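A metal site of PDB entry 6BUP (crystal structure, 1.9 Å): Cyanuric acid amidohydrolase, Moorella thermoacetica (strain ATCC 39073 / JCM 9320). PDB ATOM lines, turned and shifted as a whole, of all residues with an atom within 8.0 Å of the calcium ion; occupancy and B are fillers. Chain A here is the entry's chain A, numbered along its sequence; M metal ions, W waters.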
ATOM      1  N   TRP A 222       3.236   4.239 -10.086  1.00  0.00           N
ATOM      2  CA  TRP A 222       4.325   5.148 -10.442  1.00  0.00           C
ATOM      3  C   TRP A 222       5.311   5.364  -9.302  1.00  0.00           C
ATOM      4  O   TRP A 222       6.371   5.959  -9.490  1.00  0.00           O
ATOM      5  CB  TRP A 222       3.752   6.495 -10.892  1.00  0.00           C
ATOM      6  CG  TRP A 222       2.865   6.412 -12.083  1.00  0.00           C
ATOM      7  CD1 TRP A 222       1.584   6.915 -12.211  1.00  0.00           C
ATOM      8  CD2 TRP A 222       3.190   5.810 -13.333  1.00  0.00           C
ATOM      9  NE1 TRP A 222       1.097   6.642 -13.470  1.00  0.00           N
ATOM     10  CE2 TRP A 222       2.056   5.959 -14.181  1.00  0.00           C
ATOM     11  CE3 TRP A 222       4.305   5.134 -13.824  1.00  0.00           C
ATOM     12  CZ2 TRP A 222       2.024   5.472 -15.484  1.00  0.00           C
ATOM     13  CZ3 TRP A 222       4.268   4.639 -15.127  1.00  0.00           C
ATOM     14  CH2 TRP A 222       3.127   4.836 -15.940  1.00  0.00           C
ATOM     15  N   LEU A 224       6.886   2.924  -8.119  1.00  0.00           N
ATOM     16  CA  LEU A 224       7.948   1.986  -8.461  1.00  0.00           C
ATOM     17  C   LEU A 224       8.800   2.608  -9.550  1.00  0.00           C
ATOM     18  O   LEU A 224       8.324   2.797 -10.673  1.00  0.00           O
ATOM     19  CB  LEU A 224       7.378   0.647  -8.928  1.00  0.00           C
ATOM     20  CG  LEU A 224       6.472  -0.115  -7.950  1.00  0.00           C
ATOM     21  CD1 LEU A 224       5.862  -1.331  -8.626  1.00  0.00           C
ATOM     22  CD2 LEU A 224       7.188  -0.555  -6.682  1.00  0.00           C
ATOM     23  N   TYR A 225      10.076   2.842  -9.275  1.00  0.00           N
ATOM     24  CA  TYR A 225      10.879   3.322 -10.383  1.00  0.00           C
ATOM     25  C   TYR A 225      12.361   3.116 -10.128  1.00  0.00           C
ATOM     26  O   TYR A 225      12.797   3.047  -8.981  1.00  0.00           O
ATOM     27  CB  TYR A 225      10.626   4.811 -10.666  1.00  0.00           C
ATOM     28  CG  TYR A 225      10.855   5.780  -9.505  1.00  0.00           C
ATOM     29  CD1 TYR A 225      12.082   6.352  -9.288  1.00  0.00           C
ATOM     30  CD2 TYR A 225       9.823   6.182  -8.692  1.00  0.00           C
ATOM     31  CE1 TYR A 225      12.286   7.269  -8.270  1.00  0.00           C
ATOM     32  CE2 TYR A 225      10.024   7.078  -7.662  1.00  0.00           C
ATOM     33  CZ  TYR A 225      11.249   7.610  -7.469  1.00  0.00           C
ATOM     34  OH  TYR A 225      11.419   8.510  -6.479  1.00  0.00           O
ATOM     35  N   SER A 226      13.113   3.063 -11.220  1.00  0.00           N
ATOM     36  CA  SER A 226      14.567   3.198 -11.235  1.00  0.00           C
ATOM     37  C   SER A 226      14.974   4.675 -11.291  1.00  0.00           C
ATOM     38  O   SER A 226      14.327   5.495 -11.948  1.00  0.00           O
ATOM     39  CB  SER A 226      15.126   2.478 -12.462  1.00  0.00           C
ATOM     40  OG  SER A 226      16.511   2.730 -12.695  1.00  0.00           O
ATOM     41  N   ALA A 229      17.445   4.440 -14.922  1.00  0.00           N
ATOM     42  CA  ALA A 229      16.986   3.861 -16.177  1.00  0.00           C
ATOM     43  C   ALA A 229      16.524   4.935 -17.146  1.00  0.00           C
ATOM     44  O   ALA A 229      15.881   5.913 -16.754  1.00  0.00           O
ATOM     45  CB  ALA A 229      15.840   2.876 -15.932  1.00  0.00           C
ATOM     46  N   VAL A 261      18.145  13.153 -10.274  1.00  0.00           N
ATOM     47  CA  VAL A 261      16.799  12.859 -10.793  1.00  0.00           C
ATOM     48  C   VAL A 261      15.992  14.144 -10.797  1.00  0.00           C
ATOM     49  O   VAL A 261      15.836  14.768  -9.744  1.00  0.00           O
ATOM     50  CB  VAL A 261      16.091  11.770  -9.951  1.00  0.00           C
ATOM     51  CG1 VAL A 261      14.708  11.471 -10.509  1.00  0.00           C
ATOM     52  CG2 VAL A 261      16.948  10.496  -9.878  1.00  0.00           C
ATOM     53  N   MET A 262      15.478  14.517 -11.957  1.00  0.00           N
ATOM     54  CA  MET A 262      14.571  15.655 -12.019  1.00  0.00           C
ATOM     55  C   MET A 262      13.248  15.284 -11.375  1.00  0.00           C
ATOM     56  O   MET A 262      12.620  14.285 -11.770  1.00  0.00           O
ATOM     57  CB  MET A 262      14.338  16.092 -13.464  1.00  0.00           C
ATOM     58  CG  MET A 262      15.596  16.441 -14.236  1.00  0.00           C
ATOM     59  SD  MET A 262      15.300  17.089 -15.902  1.00  0.00           S
ATOM     60  CE  MET A 262      14.532  18.690 -15.619  1.00  0.00           C
ATOM     61  N   LYS A 263      12.814  16.062 -10.391  1.00  0.00           N
ATOM     62  CA  LYS A 263      11.550  15.771  -9.759  1.00  0.00           C
ATOM     63  C   LYS A 263      10.386  16.186 -10.635  1.00  0.00           C
ATOM     64  O   LYS A 263       9.285  15.668 -10.467  1.00  0.00           O
ATOM     65  CB  LYS A 263      11.464  16.463  -8.403  1.00  0.00           C
ATOM     66  CG  LYS A 263      11.390  17.954  -8.466  1.00  0.00           C
ATOM     67  CD  LYS A 263      11.678  18.552  -7.090  1.00  0.00           C
ATOM     68  CE  LYS A 263      11.558  20.074  -7.085  1.00  0.00           C
ATOM     69  NZ  LYS A 263      12.074  20.667  -5.802  1.00  0.00           N
ATOM     70  N   LYS A 295      15.814  11.942 -19.157  1.00  0.00           N
ATOM     71  CA  LYS A 295      14.451  11.533 -19.447  1.00  0.00           C
ATOM     72  C   LYS A 295      13.465  12.632 -19.079  1.00  0.00           C
ATOM     73  O   LYS A 295      13.641  13.318 -18.068  1.00  0.00           O
ATOM     74  CB  LYS A 295      14.091  10.265 -18.684  1.00  0.00           C
ATOM     75  CG  LYS A 295      14.804   9.011 -19.168  1.00  0.00           C
ATOM     76  CD  LYS A 295      14.395   8.620 -20.583  1.00  0.00           C
ATOM     77  CE  LYS A 295      12.873   8.606 -20.756  1.00  0.00           C
ATOM     78  NZ  LYS A 295      12.521   7.933 -22.029  1.00  0.00           N
ATOM     79  N   ALA A 296      12.431  12.789 -19.888  1.00  0.00           N
ATOM     80  CA  ALA A 296      11.405  13.825 -19.713  1.00  0.00           C
ATOM     81  C   ALA A 296      10.015  13.210 -19.841  1.00  0.00           C
ATOM     82  O   ALA A 296       9.823  12.273 -20.613  1.00  0.00           O
ATOM     83  CB  ALA A 296      11.565  14.925 -20.812  1.00  0.00           C
ATOM     84  N   GLU A 297       9.023  13.787 -19.165  1.00  0.00           N
ATOM     85  CA  GLU A 297       7.662  13.288 -19.381  1.00  0.00           C
ATOM     86  C   GLU A 297       6.605  14.240 -18.840  1.00  0.00           C
ATOM     87  O   GLU A 297       6.857  15.052 -17.949  1.00  0.00           O
ATOM     88  CB  GLU A 297       7.455  11.890 -18.743  1.00  0.00           C
ATOM     89  CG  GLU A 297       7.234  11.931 -17.231  1.00  0.00           C
ATOM     90  CD  GLU A 297       7.207  10.526 -16.604  1.00  0.00           C
ATOM     91  OE1 GLU A 297       6.858   9.551 -17.308  1.00  0.00           O
ATOM     92  OE2 GLU A 297       7.532  10.412 -15.389  1.00  0.00           O
ATOM     93  N   ALA A 298       5.396  14.067 -19.377  1.00  0.00           N
ATOM     94  CA  ALA A 298       4.183  14.648 -18.831  1.00  0.00           C
ATOM     95  C   ALA A 298       3.811  13.931 -17.541  1.00  0.00           C
ATOM     96  O   ALA A 298       3.829  12.703 -17.496  1.00  0.00           O
ATOM     97  CB  ALA A 298       3.043  14.530 -19.822  1.00  0.00           C
ATOM     98  N   ALA A 299       3.490  14.684 -16.504  1.00  0.00           N
ATOM     99  CA  ALA A 299       3.009  14.102 -15.263  1.00  0.00           C
ATOM    100  C   ALA A 299       1.587  13.591 -15.436  1.00  0.00           C
ATOM    101  O   ALA A 299       0.765  14.197 -16.131  1.00  0.00           O
ATOM    102  CB  ALA A 299       3.049  15.131 -14.129  1.00  0.00           C
ATOM    103  N   GLY A 345       9.028  10.072 -22.247  1.00  0.00           N
ATOM    104  CA  GLY A 345       8.296   8.920 -21.770  1.00  0.00           C
ATOM    105  C   GLY A 345       9.091   8.315 -20.631  1.00  0.00           C
ATOM    106  O   GLY A 345       9.991   7.507 -20.888  1.00  0.00           O
ATOM    107  N   ALA A 346       8.798   8.670 -19.375  1.00  0.00           N
ATOM    108  CA  ALA A 346       9.641   8.198 -18.276  1.00  0.00           C
ATOM    109  C   ALA A 346       8.920   7.316 -17.282  1.00  0.00           C
ATOM    110  O   ALA A 346       9.035   7.480 -16.064  1.00  0.00           O
ATOM    111  CB  ALA A 346      10.276   9.403 -17.557  1.00  0.00           C
ATOM    112  N   GLU A 347       8.162   6.377 -17.825  1.00  0.00           N
ATOM    113  CA  GLU A 347       7.442   5.402 -17.030  1.00  0.00           C
ATOM    114  C   GLU A 347       8.409   4.587 -16.196  1.00  0.00           C
ATOM    115  O   GLU A 347       9.286   3.916 -16.736  1.00  0.00           O
ATOM    116  CB  GLU A 347       6.638   4.487 -17.960  1.00  0.00           C
ATOM    117  CG  GLU A 347       5.564   5.261 -18.757  1.00  0.00           C
ATOM    118  CD  GLU A 347       6.048   5.944 -20.063  1.00  0.00           C
ATOM    119  OE1 GLU A 347       7.222   5.832 -20.424  1.00  0.00           O
ATOM    120  OE2 GLU A 347       5.222   6.580 -20.742  1.00  0.00           O
ATOM    121  N   HIS A 348       8.215   4.604 -14.883  1.00  0.00           N
ATOM    122  CA  HIS A 348       9.110   3.905 -13.964  1.00  0.00           C
ATOM    123  C   HIS A 348      10.587   4.314 -14.110  1.00  0.00           C
ATOM    124  O   HIS A 348      11.501   3.551 -13.768  1.00  0.00           O
ATOM    125  CB  HIS A 348       8.958   2.398 -14.109  1.00  0.00           C
ATOM    126  CG  HIS A 348       7.536   1.939 -14.017  1.00  0.00           C
ATOM    127  ND1 HIS A 348       6.806   1.964 -12.850  1.00  0.00           N
ATOM    128  CD2 HIS A 348       6.718   1.431 -14.965  1.00  0.00           C
ATOM    129  CE1 HIS A 348       5.603   1.461 -13.067  1.00  0.00           C
ATOM    130  NE2 HIS A 348       5.527   1.121 -14.351  1.00  0.00           N
ATOM    131  N   GLN A 349      10.800   5.533 -14.591  1.00  0.00           N
ATOM    132  CA  GLN A 349      12.116   6.153 -14.695  1.00  0.00           C
ATOM    133  C   GLN A 349      11.992   7.457 -13.932  1.00  0.00           C
ATOM    134  O   GLN A 349      11.448   8.422 -14.459  1.00  0.00           O
ATOM    135  CB  GLN A 349      12.512   6.417 -16.142  1.00  0.00           C
ATOM    136  CG  GLN A 349      12.530   5.128 -16.987  1.00  0.00           C
ATOM    137  CD  GLN A 349      12.241   5.414 -18.460  1.00  0.00           C
ATOM    138  OE1 GLN A 349      13.072   5.985 -19.168  1.00  0.00           O
ATOM    139  NE2 GLN A 349      11.061   5.033 -18.917  1.00  0.00           N
ATOM    140  N   GLY A 350      12.506   7.505 -12.712  1.00  0.00           N
ATOM    141  CA  GLY A 350      12.220   8.633 -11.830  1.00  0.00           C
ATOM    142  C   GLY A 350      10.735   8.721 -11.483  1.00  0.00           C
ATOM    143  O   GLY A 350       9.896   7.980 -12.013  1.00  0.00           O
ATOM    144  N   PRO A 351      10.381   9.649 -10.602  1.00  0.00           N
ATOM    145  CA  PRO A 351       8.973   9.768 -10.179  1.00  0.00           C
ATOM    146  C   PRO A 351       8.055  10.199 -11.332  1.00  0.00           C
ATOM    147  O   PRO A 351       8.505  10.514 -12.434  1.00  0.00           O
ATOM    148  CB  PRO A 351       9.022  10.825  -9.059  1.00  0.00           C
ATOM    149  CG  PRO A 351      10.231  11.657  -9.435  1.00  0.00           C
ATOM    150  CD  PRO A 351      11.229  10.702 -10.026  1.00  0.00           C
ATOM    151  N   ASP A 352       6.747  10.196 -11.065  1.00  0.00           N
ATOM    152  CA  ASP A 352       5.709  10.568 -12.036  1.00  0.00           C
ATOM    153  C   ASP A 352       5.892  12.037 -12.401  1.00  0.00           C
ATOM    154  O   ASP A 352       5.739  12.914 -11.546  1.00  0.00           O
ATOM    155  CB  ASP A 352       4.366  10.274 -11.383  1.00  0.00           C
ATOM    156  CG  ASP A 352       3.174  10.654 -12.222  1.00  0.00           C
ATOM    157  OD1 ASP A 352       3.337  11.044 -13.382  1.00  0.00           O
ATOM    158  OD2 ASP A 352       2.059  10.527 -11.676  1.00  0.00           O
ATOM    159  N   GLY A 353       6.277  12.329 -13.640  1.00  0.00           N
ATOM    160  CA  GLY A 353       6.576  13.697 -14.032  1.00  0.00           C
ATOM    161  C   GLY A 353       8.049  14.064 -14.061  1.00  0.00           C
ATOM    162  O   GLY A 353       8.398  15.140 -14.584  1.00  0.00           O
ATOM    163  N   GLY A 354       8.907  13.192 -13.551  1.00  0.00           N
ATOM    164  CA  GLY A 354      10.332  13.423 -13.570  1.00  0.00           C
ATOM    165  C   GLY A 354      11.075  12.257 -14.229  1.00  0.00           C
ATOM    166  O   GLY A 354      10.462  11.318 -14.733  1.00  0.00           O
ATOM    167  N   GLY A 355      12.375  12.372 -14.210  1.00  0.00           N
ATOM    168  CA  GLY A 355      13.203  11.392 -14.876  1.00  0.00           C
ATOM    169  C   GLY A 355      14.666  11.552 -14.521  1.00  0.00           C
ATOM    170  O   GLY A 355      15.111  12.627 -14.095  1.00  0.00           O
ATOM    171  N   PRO A 356      15.432  10.483 -14.679  1.00  0.00           N
ATOM    172  CA  PRO A 356      16.863  10.559 -14.373  1.00  0.00           C
ATOM    173  C   PRO A 356      17.582  11.512 -15.316  1.00  0.00           C
ATOM    174  O   PRO A 356      17.191  11.695 -16.480  1.00  0.00           O
ATOM    175  CB  PRO A 356      17.360   9.107 -14.573  1.00  0.00           C
ATOM    176  CG  PRO A 356      16.121   8.262 -14.508  1.00  0.00           C
ATOM    177  CD  PRO A 356      15.026   9.119 -15.104  1.00  0.00           C
HETATM  178 CA    CA M   1       9.120   9.220 -14.305  1.00  0.00          CA
HETATM  179  O   HOH W   1       7.104   7.873 -13.715  1.00  0.00           O
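The side-chain carboxylate of Glu 297 sits close to the backbone NH of Gly 353. The side-chain carboxylate (OE1) of Glu 297 sits at hydrogen-bond distance from the backbone NH (N) of Glu 347, 3.5 Å away. The backbone carbonyl oxygen (O) of Ser 226 sits at hydrogen-bond distance from the backbone NH (N) of Gly 350, 2.8 Å away. The backbone carbonyl oxygen of Glu 347 lies within hydrogen-bond range of the side-chain amide nitrogen of Gln 349, 3.0 Å away. The side-chain amide nitrogen (NE2) of Gln 349 lies within hydrogen-bond range of the backbone carbonyl oxygen (O) of Gly 345.
Of the 25 residues printed, 6 come within 4 Å of the calcium ion. The nearest printed residue that does not touch the calcium ion is Asp 352 (4.1 Å).
The calcium ion is bound by OE2 of Glu 297 (2.3 Å), O of Pro 351 (2.4 Å), O of Gln 349 (2.5 Å), O of Ala 346 (2.5 Å), water W1 (2.5 Å), O of Gly 354 (2.5 Å) and O of Gly 350 (2.7 Å).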
